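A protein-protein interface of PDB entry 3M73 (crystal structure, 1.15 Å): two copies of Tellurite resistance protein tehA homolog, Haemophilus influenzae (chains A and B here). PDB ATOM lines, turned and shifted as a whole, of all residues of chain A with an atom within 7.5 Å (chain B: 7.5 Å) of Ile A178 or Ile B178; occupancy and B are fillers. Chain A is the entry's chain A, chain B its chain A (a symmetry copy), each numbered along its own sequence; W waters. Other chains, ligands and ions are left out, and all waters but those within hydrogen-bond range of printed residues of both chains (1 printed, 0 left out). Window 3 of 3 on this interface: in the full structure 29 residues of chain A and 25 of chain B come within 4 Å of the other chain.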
ATOM      1  N   TYR A 143      19.886  28.666   3.187  1.00  0.00           N
ATOM      2  CA  TYR A 143      19.299  27.829   4.220  1.00  0.00           C
ATOM      3  C   TYR A 143      18.572  28.618   5.302  1.00  0.00           C
ATOM      4  O   TYR A 143      17.696  28.069   5.959  1.00  0.00           O
ATOM      5  CB  TYR A 143      20.356  26.976   4.936  1.00  0.00           C
ATOM      6  CG  TYR A 143      20.968  25.847   4.133  1.00  0.00           C
ATOM      7  CD1 TYR A 143      20.156  24.994   3.433  1.00  0.00           C
ATOM      8  CD2 TYR A 143      22.325  25.627   4.114  1.00  0.00           C
ATOM      9  CE1 TYR A 143      20.641  23.975   2.706  1.00  0.00           C
ATOM     10  CE2 TYR A 143      22.848  24.527   3.405  1.00  0.00           C
ATOM     11  CZ  TYR A 143      21.950  23.731   2.717  1.00  0.00           C
ATOM     12  OH  TYR A 143      22.335  22.666   1.929  1.00  0.00           O
ATOM     13  N   VAL A 147      15.046  26.947   5.333  1.00  0.00           N
ATOM     14  CA  VAL A 147      15.208  25.733   6.136  1.00  0.00           C
ATOM     15  C   VAL A 147      15.188  26.098   7.612  1.00  0.00           C
ATOM     16  O   VAL A 147      14.289  25.676   8.348  1.00  0.00           O
ATOM     17  CB  VAL A 147      16.487  24.996   5.737  1.00  0.00           C
ATOM     18  CG1 VAL A 147      16.713  23.818   6.645  1.00  0.00           C
ATOM     19  CG2 VAL A 147      16.379  24.538   4.286  1.00  0.00           C
ATOM     20  N   PHE A 151      12.332  25.183  10.642  1.00  0.00           N
ATOM     21  CA  PHE A 151      12.630  24.348  11.806  1.00  0.00           C
ATOM     22  C   PHE A 151      12.419  25.093  13.124  1.00  0.00           C
ATOM     23  O   PHE A 151      11.971  24.515  14.099  1.00  0.00           O
ATOM     24  CB  PHE A 151      14.043  23.796  11.749  1.00  0.00           C
ATOM     25  CG  PHE A 151      14.285  22.770  10.658  1.00  0.00           C
ATOM     26  CD1 PHE A 151      13.333  21.839  10.334  1.00  0.00           C
ATOM     27  CD2 PHE A 151      15.519  22.706  10.039  1.00  0.00           C
ATOM     28  CE1 PHE A 151      13.589  20.880   9.377  1.00  0.00           C
ATOM     29  CE2 PHE A 151      15.783  21.747   9.096  1.00  0.00           C
ATOM     30  CZ  PHE A 151      14.818  20.831   8.764  1.00  0.00           C
ATOM     31  N   ALA A 172       8.103  21.310   5.936  1.00  0.00           N
ATOM     32  CA  ALA A 172       8.506  22.344   5.022  1.00  0.00           C
ATOM     33  C   ALA A 172      10.020  22.524   5.060  1.00  0.00           C
ATOM     34  O   ALA A 172      10.672  22.607   4.023  1.00  0.00           O
ATOM     35  CB  ALA A 172       7.768  23.642   5.334  1.00  0.00           C
ATOM     36  N   GLY A 173      10.587  22.631   6.261  1.00  0.00           N
ATOM     37  CA  GLY A 173      12.022  22.809   6.364  1.00  0.00           C
ATOM     38  C   GLY A 173      12.845  21.631   5.899  1.00  0.00           C
ATOM     39  O   GLY A 173      13.879  21.795   5.265  1.00  0.00           O
ATOM     40  N   MET A 174      12.415  20.432   6.260  1.00  0.00           N
ATOM     41  CA  MET A 174      13.191  19.241   5.928  1.00  0.00           C
ATOM     42  C   MET A 174      13.209  18.993   4.423  1.00  0.00           C
ATOM     43  O   MET A 174      14.264  18.668   3.867  1.00  0.00           O
ATOM     44  CB  MET A 174      12.617  18.040   6.682  1.00  0.00           C
ATOM     45  CG  MET A 174      13.466  16.781   6.439  1.00  0.00           C
ATOM     46  SD  MET A 174      12.842  15.367   7.377  1.00  0.00           S
ATOM     47  CE  MET A 174      13.961  14.132   6.738  1.00  0.00           C
ATOM     48  N   ILE A 175      12.044  19.061   3.786  1.00  0.00           N
ATOM     49  CA  ILE A 175      12.016  18.850   2.359  1.00  0.00           C
ATOM     50  C   ILE A 175      12.707  20.016   1.642  1.00  0.00           C
ATOM     51  O   ILE A 175      13.439  19.787   0.683  1.00  0.00           O
ATOM     52  CB  ILE A 175      10.591  18.517   1.879  1.00  0.00           C
ATOM     53  CG1 ILE A 175      10.152  17.180   2.519  1.00  0.00           C
ATOM     54  CG2 ILE A 175      10.553  18.416   0.361  1.00  0.00           C
ATOM     55  CD1 ILE A 175       8.725  16.799   2.272  1.00  0.00           C
ATOM     56  N   ALA A 176      12.526  21.263   2.097  1.00  0.00           N
ATOM     57  CA  ALA A 176      13.233  22.368   1.470  1.00  0.00           C
ATOM     58  C   ALA A 176      14.737  22.155   1.533  1.00  0.00           C
ATOM     59  O   ALA A 176      15.448  22.538   0.598  1.00  0.00           O
ATOM     60  CB  ALA A 176      12.849  23.688   2.094  1.00  0.00           C
ATOM     61  N   TRP A 177      15.241  21.623   2.654  1.00  0.00           N
ATOM     62  CA  TRP A 177      16.676  21.359   2.804  1.00  0.00           C
ATOM     63  C   TRP A 177      17.169  20.357   1.758  1.00  0.00           C
ATOM     64  O   TRP A 177      18.126  20.629   1.030  1.00  0.00           O
ATOM     65  CB  TRP A 177      16.887  20.802   4.210  1.00  0.00           C
ATOM     66  CG  TRP A 177      18.220  20.119   4.418  1.00  0.00           C
ATOM     67  CD1 TRP A 177      19.422  20.414   3.846  1.00  0.00           C
ATOM     68  CD2 TRP A 177      18.442  18.962   5.234  1.00  0.00           C
ATOM     69  NE1 TRP A 177      20.375  19.513   4.248  1.00  0.00           N
ATOM     70  CE2 TRP A 177      19.796  18.613   5.100  1.00  0.00           C
ATOM     71  CE3 TRP A 177      17.627  18.196   6.075  1.00  0.00           C
ATOM     72  CZ2 TRP A 177      20.339  17.518   5.758  1.00  0.00           C
ATOM     73  CZ3 TRP A 177      18.163  17.098   6.706  1.00  0.00           C
ATOM     74  CH2 TRP A 177      19.510  16.797   6.567  1.00  0.00           C
ATOM     75  N   ILE A 178      16.498  19.225   1.689  1.00  0.00           N
ATOM     76  CA  ILE A 178      16.898  18.181   0.774  1.00  0.00           C
ATOM     77  C   ILE A 178      16.784  18.654  -0.675  1.00  0.00           C
ATOM     78  O   ILE A 178      17.518  18.186  -1.535  1.00  0.00           O
ATOM     79  CB  ILE A 178      16.074  16.900   1.066  1.00  0.00           C
ATOM     80  CG1 ILE A 178      16.362  16.413   2.479  1.00  0.00           C
ATOM     81  CG2 ILE A 178      16.262  15.843  -0.043  1.00  0.00           C
ATOM     82  CD1 ILE A 178      17.752  16.116   2.802  1.00  0.00           C
ATOM     83  N   ILE A 179      15.853  19.578  -0.944  1.00  0.00           N
ATOM     84  CA  ILE A 179      15.686  20.097  -2.287  1.00  0.00           C
ATOM     85  C   ILE A 179      16.732  21.147  -2.689  1.00  0.00           C
ATOM     86  O   ILE A 179      17.038  21.275  -3.860  1.00  0.00           O
ATOM     87  CB  ILE A 179      14.229  20.602  -2.479  1.00  0.00           C
ATOM     88  CG1 ILE A 179      13.222  19.459  -2.284  1.00  0.00           C
ATOM     89  CG2 ILE A 179      14.000  21.192  -3.832  1.00  0.00           C
ATOM     90  CD1 ILE A 179      13.432  18.274  -3.044  1.00  0.00           C
ATOM     91  N   PHE A 180      17.276  21.879  -1.711  1.00  0.00           N
ATOM     92  CA  PHE A 180      18.301  22.867  -2.006  1.00  0.00           C
ATOM     93  C   PHE A 180      19.728  22.326  -1.974  1.00  0.00           C
ATOM     94  O   PHE A 180      20.541  22.638  -2.839  1.00  0.00           O
ATOM     95  CB  PHE A 180      18.194  24.074  -1.062  1.00  0.00           C
ATOM     96  CG  PHE A 180      19.209  25.160  -1.384  1.00  0.00           C
ATOM     97  CD1 PHE A 180      19.115  25.842  -2.571  1.00  0.00           C
ATOM     98  CD2 PHE A 180      20.258  25.453  -0.550  1.00  0.00           C
ATOM     99  CE1 PHE A 180      19.976  26.849  -2.894  1.00  0.00           C
ATOM    100  CE2 PHE A 180      21.174  26.512  -0.920  1.00  0.00           C
ATOM    101  CZ  PHE A 180      20.977  27.135  -2.075  1.00  0.00           C
ATOM    102  N   GLU A 181      20.042  21.536  -0.950  1.00  0.00           N
ATOM    103  CA  GLU A 181      21.409  21.100  -0.790  1.00  0.00           C
ATOM    104  C   GLU A 181      22.033  20.482  -2.042  1.00  0.00           C
ATOM    105  O   GLU A 181      23.231  20.701  -2.271  1.00  0.00           O
ATOM    106  CB  GLU A 181      21.576  20.214   0.446  1.00  0.00           C
ATOM    107  CG  GLU A 181      23.027  19.936   0.756  1.00  0.00           C
ATOM    108  CD  GLU A 181      23.298  19.657   2.232  1.00  0.00           C
ATOM    109  OE1 GLU A 181      23.970  18.643   2.482  1.00  0.00           O
ATOM    110  OE2 GLU A 181      22.848  20.421   3.096  1.00  0.00           O
ATOM    111  N   PRO A 182      21.317  19.688  -2.855  1.00  0.00           N
ATOM    112  CA  PRO A 182      21.990  19.080  -4.013  1.00  0.00           C
ATOM    113  C   PRO A 182      22.691  20.116  -4.888  1.00  0.00           C
ATOM    114  O   PRO A 182      23.802  19.928  -5.349  1.00  0.00           O
ATOM    115  CB  PRO A 182      20.847  18.377  -4.742  1.00  0.00           C
ATOM    116  CG  PRO A 182      19.863  18.030  -3.638  1.00  0.00           C
ATOM    117  CD  PRO A 182      19.927  19.234  -2.721  1.00  0.00           C
ATOM    118  N   VAL A 183      21.968  21.195  -5.176  1.00  0.00           N
ATOM    119  CA  VAL A 183      22.495  22.211  -6.067  1.00  0.00           C
ATOM    120  C   VAL A 183      23.546  23.059  -5.385  1.00  0.00           C
ATOM    121  O   VAL A 183      24.476  23.552  -6.042  1.00  0.00           O
ATOM    122  CB  VAL A 183      21.399  23.028  -6.789  1.00  0.00           C
ATOM    123  CG1 VAL A 183      20.526  22.076  -7.602  1.00  0.00           C
ATOM    124  CG2 VAL A 183      20.592  23.882  -5.845  1.00  0.00           C
ATOM    125  N   PRO A 207      21.926  22.207   8.703  1.00  0.00           N
ATOM    126  CA  PRO A 207      20.664  21.550   8.411  1.00  0.00           C
ATOM    127  C   PRO A 207      20.354  20.288   9.193  1.00  0.00           C
ATOM    128  O   PRO A 207      19.267  20.176   9.763  1.00  0.00           O
ATOM    129  CB  PRO A 207      20.730  21.341   6.898  1.00  0.00           C
ATOM    130  CG  PRO A 207      21.522  22.526   6.417  1.00  0.00           C
ATOM    131  CD  PRO A 207      22.577  22.715   7.484  1.00  0.00           C
ATOM    132  N   LEU A 230      19.697  11.420  10.824  1.00  0.00           N
ATOM    133  CA  LEU A 230      20.048  12.807  10.727  1.00  0.00           C
ATOM    134  C   LEU A 230      21.370  13.103  11.403  1.00  0.00           C
ATOM    135  O   LEU A 230      22.193  13.845  10.879  1.00  0.00           O
ATOM    136  CB  LEU A 230      18.931  13.666  11.335  1.00  0.00           C
ATOM    137  CG  LEU A 230      17.609  13.680  10.546  1.00  0.00           C
ATOM    138  CD1 LEU A 230      16.491  14.244  11.367  1.00  0.00           C
ATOM    139  CD2 LEU A 230      17.759  14.433   9.246  1.00  0.00           C
ATOM    140  N   TYR A 233      24.362  12.000   9.068  1.00  0.00           N
ATOM    141  CA  TYR A 233      24.731  12.959   8.040  1.00  0.00           C
ATOM    142  C   TYR A 233      25.302  14.240   8.659  1.00  0.00           C
ATOM    143  O   TYR A 233      26.247  14.813   8.139  1.00  0.00           O
ATOM    144  CB  TYR A 233      23.549  13.277   7.139  1.00  0.00           C
ATOM    145  CG  TYR A 233      23.913  14.081   5.921  1.00  0.00           C
ATOM    146  CD1 TYR A 233      24.514  13.476   4.846  1.00  0.00           C
ATOM    147  CD2 TYR A 233      23.665  15.440   5.827  1.00  0.00           C
ATOM    148  CE1 TYR A 233      24.842  14.187   3.721  1.00  0.00           C
ATOM    149  CE2 TYR A 233      24.008  16.166   4.693  1.00  0.00           C
ATOM    150  CZ  TYR A 233      24.577  15.526   3.633  1.00  0.00           C
ATOM    151  OH  TYR A 233      24.898  16.178   2.453  1.00  0.00           O
ATOM    152  N   TYR B 143       7.290  16.112 -14.009  1.00  0.00           N
ATOM    153  CA  TYR B 143       6.650  15.412 -12.910  1.00  0.00           C
ATOM    154  C   TYR B 143       5.563  14.441 -13.357  1.00  0.00           C
ATOM    155  O   TYR B 143       5.260  13.503 -12.630  1.00  0.00           O
ATOM    156  CB  TYR B 143       5.988  16.381 -11.919  1.00  0.00           C
ATOM    157  CG  TYR B 143       6.924  17.213 -11.066  1.00  0.00           C
ATOM    158  CD1 TYR B 143       7.968  16.610 -10.418  1.00  0.00           C
ATOM    159  CD2 TYR B 143       6.733  18.563 -10.891  1.00  0.00           C
ATOM    160  CE1 TYR B 143       8.827  17.295  -9.646  1.00  0.00           C
ATOM    161  CE2 TYR B 143       7.587  19.289 -10.037  1.00  0.00           C
ATOM    162  CZ  TYR B 143       8.624  18.594  -9.439  1.00  0.00           C
ATOM    163  OH  TYR B 143       9.572  19.197  -8.638  1.00  0.00           O
ATOM    164  N   VAL B 147       6.667  11.105 -11.660  1.00  0.00           N
ATOM    165  CA  VAL B 147       6.196  11.208 -10.277  1.00  0.00           C
ATOM    166  C   VAL B 147       4.710  10.891 -10.226  1.00  0.00           C
ATOM    167  O   VAL B 147       4.302   9.907  -9.598  1.00  0.00           O
ATOM    168  CB  VAL B 147       6.515  12.591  -9.706  1.00  0.00           C
ATOM    169  CG1 VAL B 147       5.922  12.735  -8.331  1.00  0.00           C
ATOM    170  CG2 VAL B 147       8.026  12.786  -9.659  1.00  0.00           C
ATOM    171  N   PHE B 151       2.650   7.605  -8.454  1.00  0.00           N
ATOM    172  CA  PHE B 151       1.711   7.747  -7.341  1.00  0.00           C
ATOM    173  C   PHE B 151       0.312   7.243  -7.693  1.00  0.00           C
ATOM    174  O   PHE B 151      -0.369   6.668  -6.861  1.00  0.00           O
ATOM    175  CB  PHE B 151       1.631   9.184  -6.858  1.00  0.00           C
ATOM    176  CG  PHE B 151       2.884   9.699  -6.174  1.00  0.00           C
ATOM    177  CD1 PHE B 151       3.623   8.895  -5.344  1.00  0.00           C
ATOM    178  CD2 PHE B 151       3.242  11.027  -6.309  1.00  0.00           C
ATOM    179  CE1 PHE B 151       4.729   9.395  -4.688  1.00  0.00           C
ATOM    180  CE2 PHE B 151       4.333  11.532  -5.650  1.00  0.00           C
ATOM    181  CZ  PHE B 151       5.078  10.715  -4.837  1.00  0.00           C
ATOM    182  N   ALA B 172       8.945   4.615  -5.913  1.00  0.00           N
ATOM    183  CA  ALA B 172       9.458   5.100  -7.165  1.00  0.00           C
ATOM    184  C   ALA B 172       9.076   6.563  -7.364  1.00  0.00           C
ATOM    185  O   ALA B 172       9.906   7.387  -7.740  1.00  0.00           O
ATOM    186  CB  ALA B 172       8.967   4.221  -8.312  1.00  0.00           C
ATOM    187  N   GLY B 173       7.802   6.891  -7.152  1.00  0.00           N
ATOM    188  CA  GLY B 173       7.376   8.265  -7.329  1.00  0.00           C
ATOM    189  C   GLY B 173       7.963   9.246  -6.341  1.00  0.00           C
ATOM    190  O   GLY B 173       8.315  10.364  -6.696  1.00  0.00           O
ATOM    191  N   MET B 174       8.021   8.848  -5.079  1.00  0.00           N
ATOM    192  CA  MET B 174       8.495   9.760  -4.042  1.00  0.00           C
ATOM    193  C   MET B 174       9.978  10.072  -4.214  1.00  0.00           C
ATOM    194  O   MET B 174      10.381  11.232  -4.077  1.00  0.00           O
ATOM    195  CB  MET B 174       8.212   9.150  -2.668  1.00  0.00           C
ATOM    196  CG  MET B 174       8.604  10.122  -1.543  1.00  0.00           C
ATOM    197  SD  MET B 174       8.213   9.445   0.086  1.00  0.00           S
ATOM    198  CE  MET B 174       8.920  10.753   1.075  1.00  0.00           C
ATOM    199  N   ILE B 175      10.791   9.042  -4.426  1.00  0.00           N
ATOM    200  CA  ILE B 175      12.200   9.292  -4.611  1.00  0.00           C
ATOM    201  C   ILE B 175      12.435  10.012  -5.944  1.00  0.00           C
ATOM    202  O   ILE B 175      13.257  10.924  -6.002  1.00  0.00           O
ATOM    203  CB  ILE B 175      13.022   8.008  -4.388  1.00  0.00           C
ATOM    204  CG1 ILE B 175      12.855   7.561  -2.919  1.00  0.00           C
ATOM    205  CG2 ILE B 175      14.489   8.257  -4.704  1.00  0.00           C
ATOM    206  CD1 ILE B 175      13.469   6.237  -2.586  1.00  0.00           C
ATOM    207  N   ALA B 176      11.713   9.658  -7.016  1.00  0.00           N
ATOM    208  CA  ALA B 176      11.876  10.382  -8.265  1.00  0.00           C
ATOM    209  C   ALA B 176      11.577  11.861  -8.078  1.00  0.00           C
ATOM    210  O   ALA B 176      12.219  12.700  -8.718  1.00  0.00           O
ATOM    211  CB  ALA B 176      11.015   9.792  -9.356  1.00  0.00           C
ATOM    212  N   TRP B 177      10.558  12.190  -7.273  1.00  0.00           N
ATOM    213  CA  TRP B 177      10.203  13.589  -7.011  1.00  0.00           C
ATOM    214  C   TRP B 177      11.357  14.339  -6.344  1.00  0.00           C
ATOM    215  O   TRP B 177      11.785  15.391  -6.826  1.00  0.00           O
ATOM    216  CB  TRP B 177       8.980  13.580  -6.098  1.00  0.00           C
ATOM    217  CG  TRP B 177       8.700  14.900  -5.414  1.00  0.00           C
ATOM    218  CD1 TRP B 177       8.927  16.160  -5.882  1.00  0.00           C
ATOM    219  CD2 TRP B 177       8.189  15.055  -4.085  1.00  0.00           C
ATOM    220  NE1 TRP B 177       8.596  17.089  -4.928  1.00  0.00           N
ATOM    221  CE2 TRP B 177       8.142  16.433  -3.817  1.00  0.00           C
ATOM    222  CE3 TRP B 177       7.758  14.160  -3.100  1.00  0.00           C
ATOM    223  CZ2 TRP B 177       7.701  16.928  -2.597  1.00  0.00           C
ATOM    224  CZ3 TRP B 177       7.343  14.653  -1.885  1.00  0.00           C
ATOM    225  CH2 TRP B 177       7.290  16.021  -1.664  1.00  0.00           C
ATOM    226  N   ILE B 178      11.852  13.779  -5.259  1.00  0.00           N
ATOM    227  CA  ILE B 178      12.912  14.418  -4.513  1.00  0.00           C
ATOM    228  C   ILE B 178      14.179  14.536  -5.359  1.00  0.00           C
ATOM    229  O   ILE B 178      14.970  15.448  -5.160  1.00  0.00           O
ATOM    230  CB  ILE B 178      13.135  13.654  -3.181  1.00  0.00           C
ATOM    231  CG1 ILE B 178      11.871  13.714  -2.335  1.00  0.00           C
ATOM    232  CG2 ILE B 178      14.423  14.122  -2.471  1.00  0.00           C
ATOM    233  CD1 ILE B 178      11.370  15.039  -1.994  1.00  0.00           C
ATOM    234  N   ILE B 179      14.373  13.603  -6.300  1.00  0.00           N
ATOM    235  CA  ILE B 179      15.539  13.646  -7.161  1.00  0.00           C
ATOM    236  C   ILE B 179      15.436  14.666  -8.305  1.00  0.00           C
ATOM    237  O   ILE B 179      16.449  15.171  -8.754  1.00  0.00           O
ATOM    238  CB  ILE B 179      15.874  12.215  -7.666  1.00  0.00           C
ATOM    239  CG1 ILE B 179      16.188  11.279  -6.489  1.00  0.00           C
ATOM    240  CG2 ILE B 179      17.042  12.194  -8.596  1.00  0.00           C
ATOM    241  CD1 ILE B 179      17.176  11.714  -5.562  1.00  0.00           C
ATOM    242  N   PHE B 180      14.212  14.965  -8.755  1.00  0.00           N
ATOM    243  CA  PHE B 180      14.030  15.949  -9.810  1.00  0.00           C
ATOM    244  C   PHE B 180      13.861  17.383  -9.314  1.00  0.00           C
ATOM    245  O   PHE B 180      14.436  18.315  -9.868  1.00  0.00           O
ATOM    246  CB  PHE B 180      12.842  15.580 -10.712  1.00  0.00           C
ATOM    247  CG  PHE B 180      12.662  16.551 -11.868  1.00  0.00           C
ATOM    248  CD1 PHE B 180      13.623  16.625 -12.844  1.00  0.00           C
ATOM    249  CD2 PHE B 180      11.590  17.405 -11.946  1.00  0.00           C
ATOM    250  CE1 PHE B 180      13.493  17.452 -13.921  1.00  0.00           C
ATOM    251  CE2 PHE B 180      11.482  18.291 -13.087  1.00  0.00           C
ATOM    252  CZ  PHE B 180      12.447  18.262 -13.996  1.00  0.00           C
ATOM    253  N   GLU B 181      13.040  17.562  -8.282  1.00  0.00           N
ATOM    254  CA  GLU B 181      12.735  18.906  -7.851  1.00  0.00           C
ATOM    255  C   GLU B 181      13.956  19.794  -7.612  1.00  0.00           C
ATOM    256  O   GLU B 181      13.880  20.993  -7.912  1.00  0.00           O
ATOM    257  CB  GLU B 181      11.766  18.910  -6.666  1.00  0.00           C
ATOM    258  CG  GLU B 181      11.261  20.297  -6.348  1.00  0.00           C
ATOM    259  CD  GLU B 181       9.887  20.312  -5.684  1.00  0.00           C
ATOM    260  OE1 GLU B 181       9.784  21.003  -4.655  1.00  0.00           O
ATOM    261  OE2 GLU B 181       8.958  19.656  -6.172  1.00  0.00           O
ATOM    262  N   PRO B 182      15.074  19.300  -7.054  1.00  0.00           N
ATOM    263  CA  PRO B 182      16.195  20.218  -6.799  1.00  0.00           C
ATOM    264  C   PRO B 182      16.611  20.988  -8.050  1.00  0.00           C
ATOM    265  O   PRO B 182      16.877  22.175  -8.021  1.00  0.00           O
ATOM    266  CB  PRO B 182      17.293  19.285  -6.295  1.00  0.00           C
ATOM    267  CG  PRO B 182      16.536  18.145  -5.638  1.00  0.00           C
ATOM    268  CD  PRO B 182      15.341  17.948  -6.548  1.00  0.00           C
ATOM    269  N   VAL B 183      16.742  20.250  -9.150  1.00  0.00           N
ATOM    270  CA  VAL B 183      17.214  20.853 -10.382  1.00  0.00           C
ATOM    271  C   VAL B 183      16.139  21.695 -11.037  1.00  0.00           C
ATOM    272  O   VAL B 183      16.447  22.690 -11.712  1.00  0.00           O
ATOM    273  CB  VAL B 183      17.896  19.850 -11.340  1.00  0.00           C
ATOM    274  CG1 VAL B 183      19.086  19.215 -10.624  1.00  0.00           C
ATOM    275  CG2 VAL B 183      16.939  18.822 -11.885  1.00  0.00           C
ATOM    276  N   PRO B 207       3.374  17.589  -6.342  1.00  0.00           N
ATOM    277  CA  PRO B 207       4.072  16.455  -5.760  1.00  0.00           C
ATOM    278  C   PRO B 207       3.725  16.104  -4.326  1.00  0.00           C
ATOM    279  O   PRO B 207       3.431  14.942  -4.038  1.00  0.00           O
ATOM    280  CB  PRO B 207       5.542  16.813  -5.973  1.00  0.00           C
ATOM    281  CG  PRO B 207       5.529  17.588  -7.263  1.00  0.00           C
ATOM    282  CD  PRO B 207       4.265  18.413  -7.177  1.00  0.00           C
ATOM    283  N   LEU B 230       4.645  15.830   4.664  1.00  0.00           N
ATOM    284  CA  LEU B 230       4.302  16.088   3.295  1.00  0.00           C
ATOM    285  C   LEU B 230       3.325  17.237   3.163  1.00  0.00           C
ATOM    286  O   LEU B 230       3.464  18.083   2.287  1.00  0.00           O
ATOM    287  CB  LEU B 230       3.722  14.816   2.660  1.00  0.00           C
ATOM    288  CG  LEU B 230       4.724  13.664   2.462  1.00  0.00           C
ATOM    289  CD1 LEU B 230       4.020  12.375   2.169  1.00  0.00           C
ATOM    290  CD2 LEU B 230       5.725  13.993   1.380  1.00  0.00           C
ATOM    291  N   TYR B 233       5.232  20.681   3.519  1.00  0.00           N
ATOM    292  CA  TYR B 233       5.878  21.159   2.308  1.00  0.00           C
ATOM    293  C   TYR B 233       4.845  21.508   1.231  1.00  0.00           C
ATOM    294  O   TYR B 233       4.999  22.486   0.516  1.00  0.00           O
ATOM    295  CB  TYR B 233       6.879  20.142   1.784  1.00  0.00           C
ATOM    296  CG  TYR B 233       7.746  20.660   0.671  1.00  0.00           C
ATOM    297  CD1 TYR B 233       8.803  21.493   0.946  1.00  0.00           C
ATOM    298  CD2 TYR B 233       7.527  20.332  -0.656  1.00  0.00           C
ATOM    299  CE1 TYR B 233       9.614  21.966  -0.052  1.00  0.00           C
ATOM    300  CE2 TYR B 233       8.340  20.821  -1.672  1.00  0.00           C
ATOM    301  CZ  TYR B 233       9.398  21.621  -1.358  1.00  0.00           C
ATOM    302  OH  TYR B 233      10.276  22.103  -2.314  1.00  0.00           O
HETATM  303  O   HOH W   1      16.760  23.496  -5.508  1.00  0.00           O
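Of the printed residues of chain B, Ala A176 touches Tyr B233 (3.7 Å).
Printed residues of chain B within 4 Å of Ile A178: Ile B178.
Of the printed residues of chain B, Ile A179 touches Ile B178 (3.9 Å), Glu B181 (3.8 Å), Pro B182 (3.2 Å) and Tyr B233 (3.96 Å).
Glu A181 touches none of the printed residues of chain B.
Of the printed residues of chain B, Val A183 touches Pro B182.
Of the printed residues of chain A, Ile B178 touches Ile A178 (3.5 Å) and Ile A179 (3.9 Å).
Printed residues of chain A within 4 Å of Tyr B233: Ala A172 (3.8 Å), Ile A175 (3.6 Å), Ala A176 (3.7 Å) and Ile A179 (3.96 Å).
The nearest printed residue of chain B that does not touch Ala A172 is Leu B230 (6.6 Å).
Hydrophobic or aromatic side chains of chain A within 4 Å of the printed part of chain B: Ile A175, Ile A178, Ile A179, Pro A182 and Val A183.
Along chain A the printed residues that touch a printed residue of chain B span positions 172 to 183.
Hydrophobic or aromatic side chains of chain B that line the printed part of chain A: Ile B178, Pro B182 and Tyr B233.
The side-chain carboxylate of Glu B181 sits at hydrogen-bond distance from the side-chain hydroxyl of Tyr B233 (2.6 Å).
NE1 of Trp B177 lies within hydrogen-bond range of OE2 of Glu B181 (2.9 Å).
OH of Tyr B143 lies within hydrogen-bond range of OE2 of Glu B181 (2.6 Å).
Ala A172 touches Tyr B233, but with the chains exchanged Tyr A233 does not touch Ala B172 (20.0 Å).
Ile A175 touches Tyr B233, but with the chains exchanged Tyr A233 does not touch Ile B175 (14.6 Å).
Ile A179 touches Glu B181, but with the chains exchanged Glu A181 does not touch Ile B179 (10.2 Å).
Ile A179 touches Tyr B233, but with the chains exchanged Tyr A233 does not touch Ile B179 (12.0 Å).
Tyr B233 touches Ala A172.
Ile A175 touches Tyr B233.
N of Ala A176 touches CE1 of Tyr B233, at 3.7 Å.
Ile B178 touches Ile A178.
Ile A179 touches Ile B178.
CG2 of Ile A179 touches CG of Glu B181, at 3.8 Å.
Ile A179 touches Pro B182 (O to CB, 3.2 Å).
Tyr B233 touches Ile A179 (OH to CG1, 3.96 Å).
Pro A182 touches Pro B182 (CG to CG, 3.9 Å).
Val A183 touches Pro B182 (CG1 to O, 3.7 Å).
Water W1 lies within hydrogen-bond range of O of Ile A179 (2.8 Å) and O of Pro B182 (2.8 Å).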
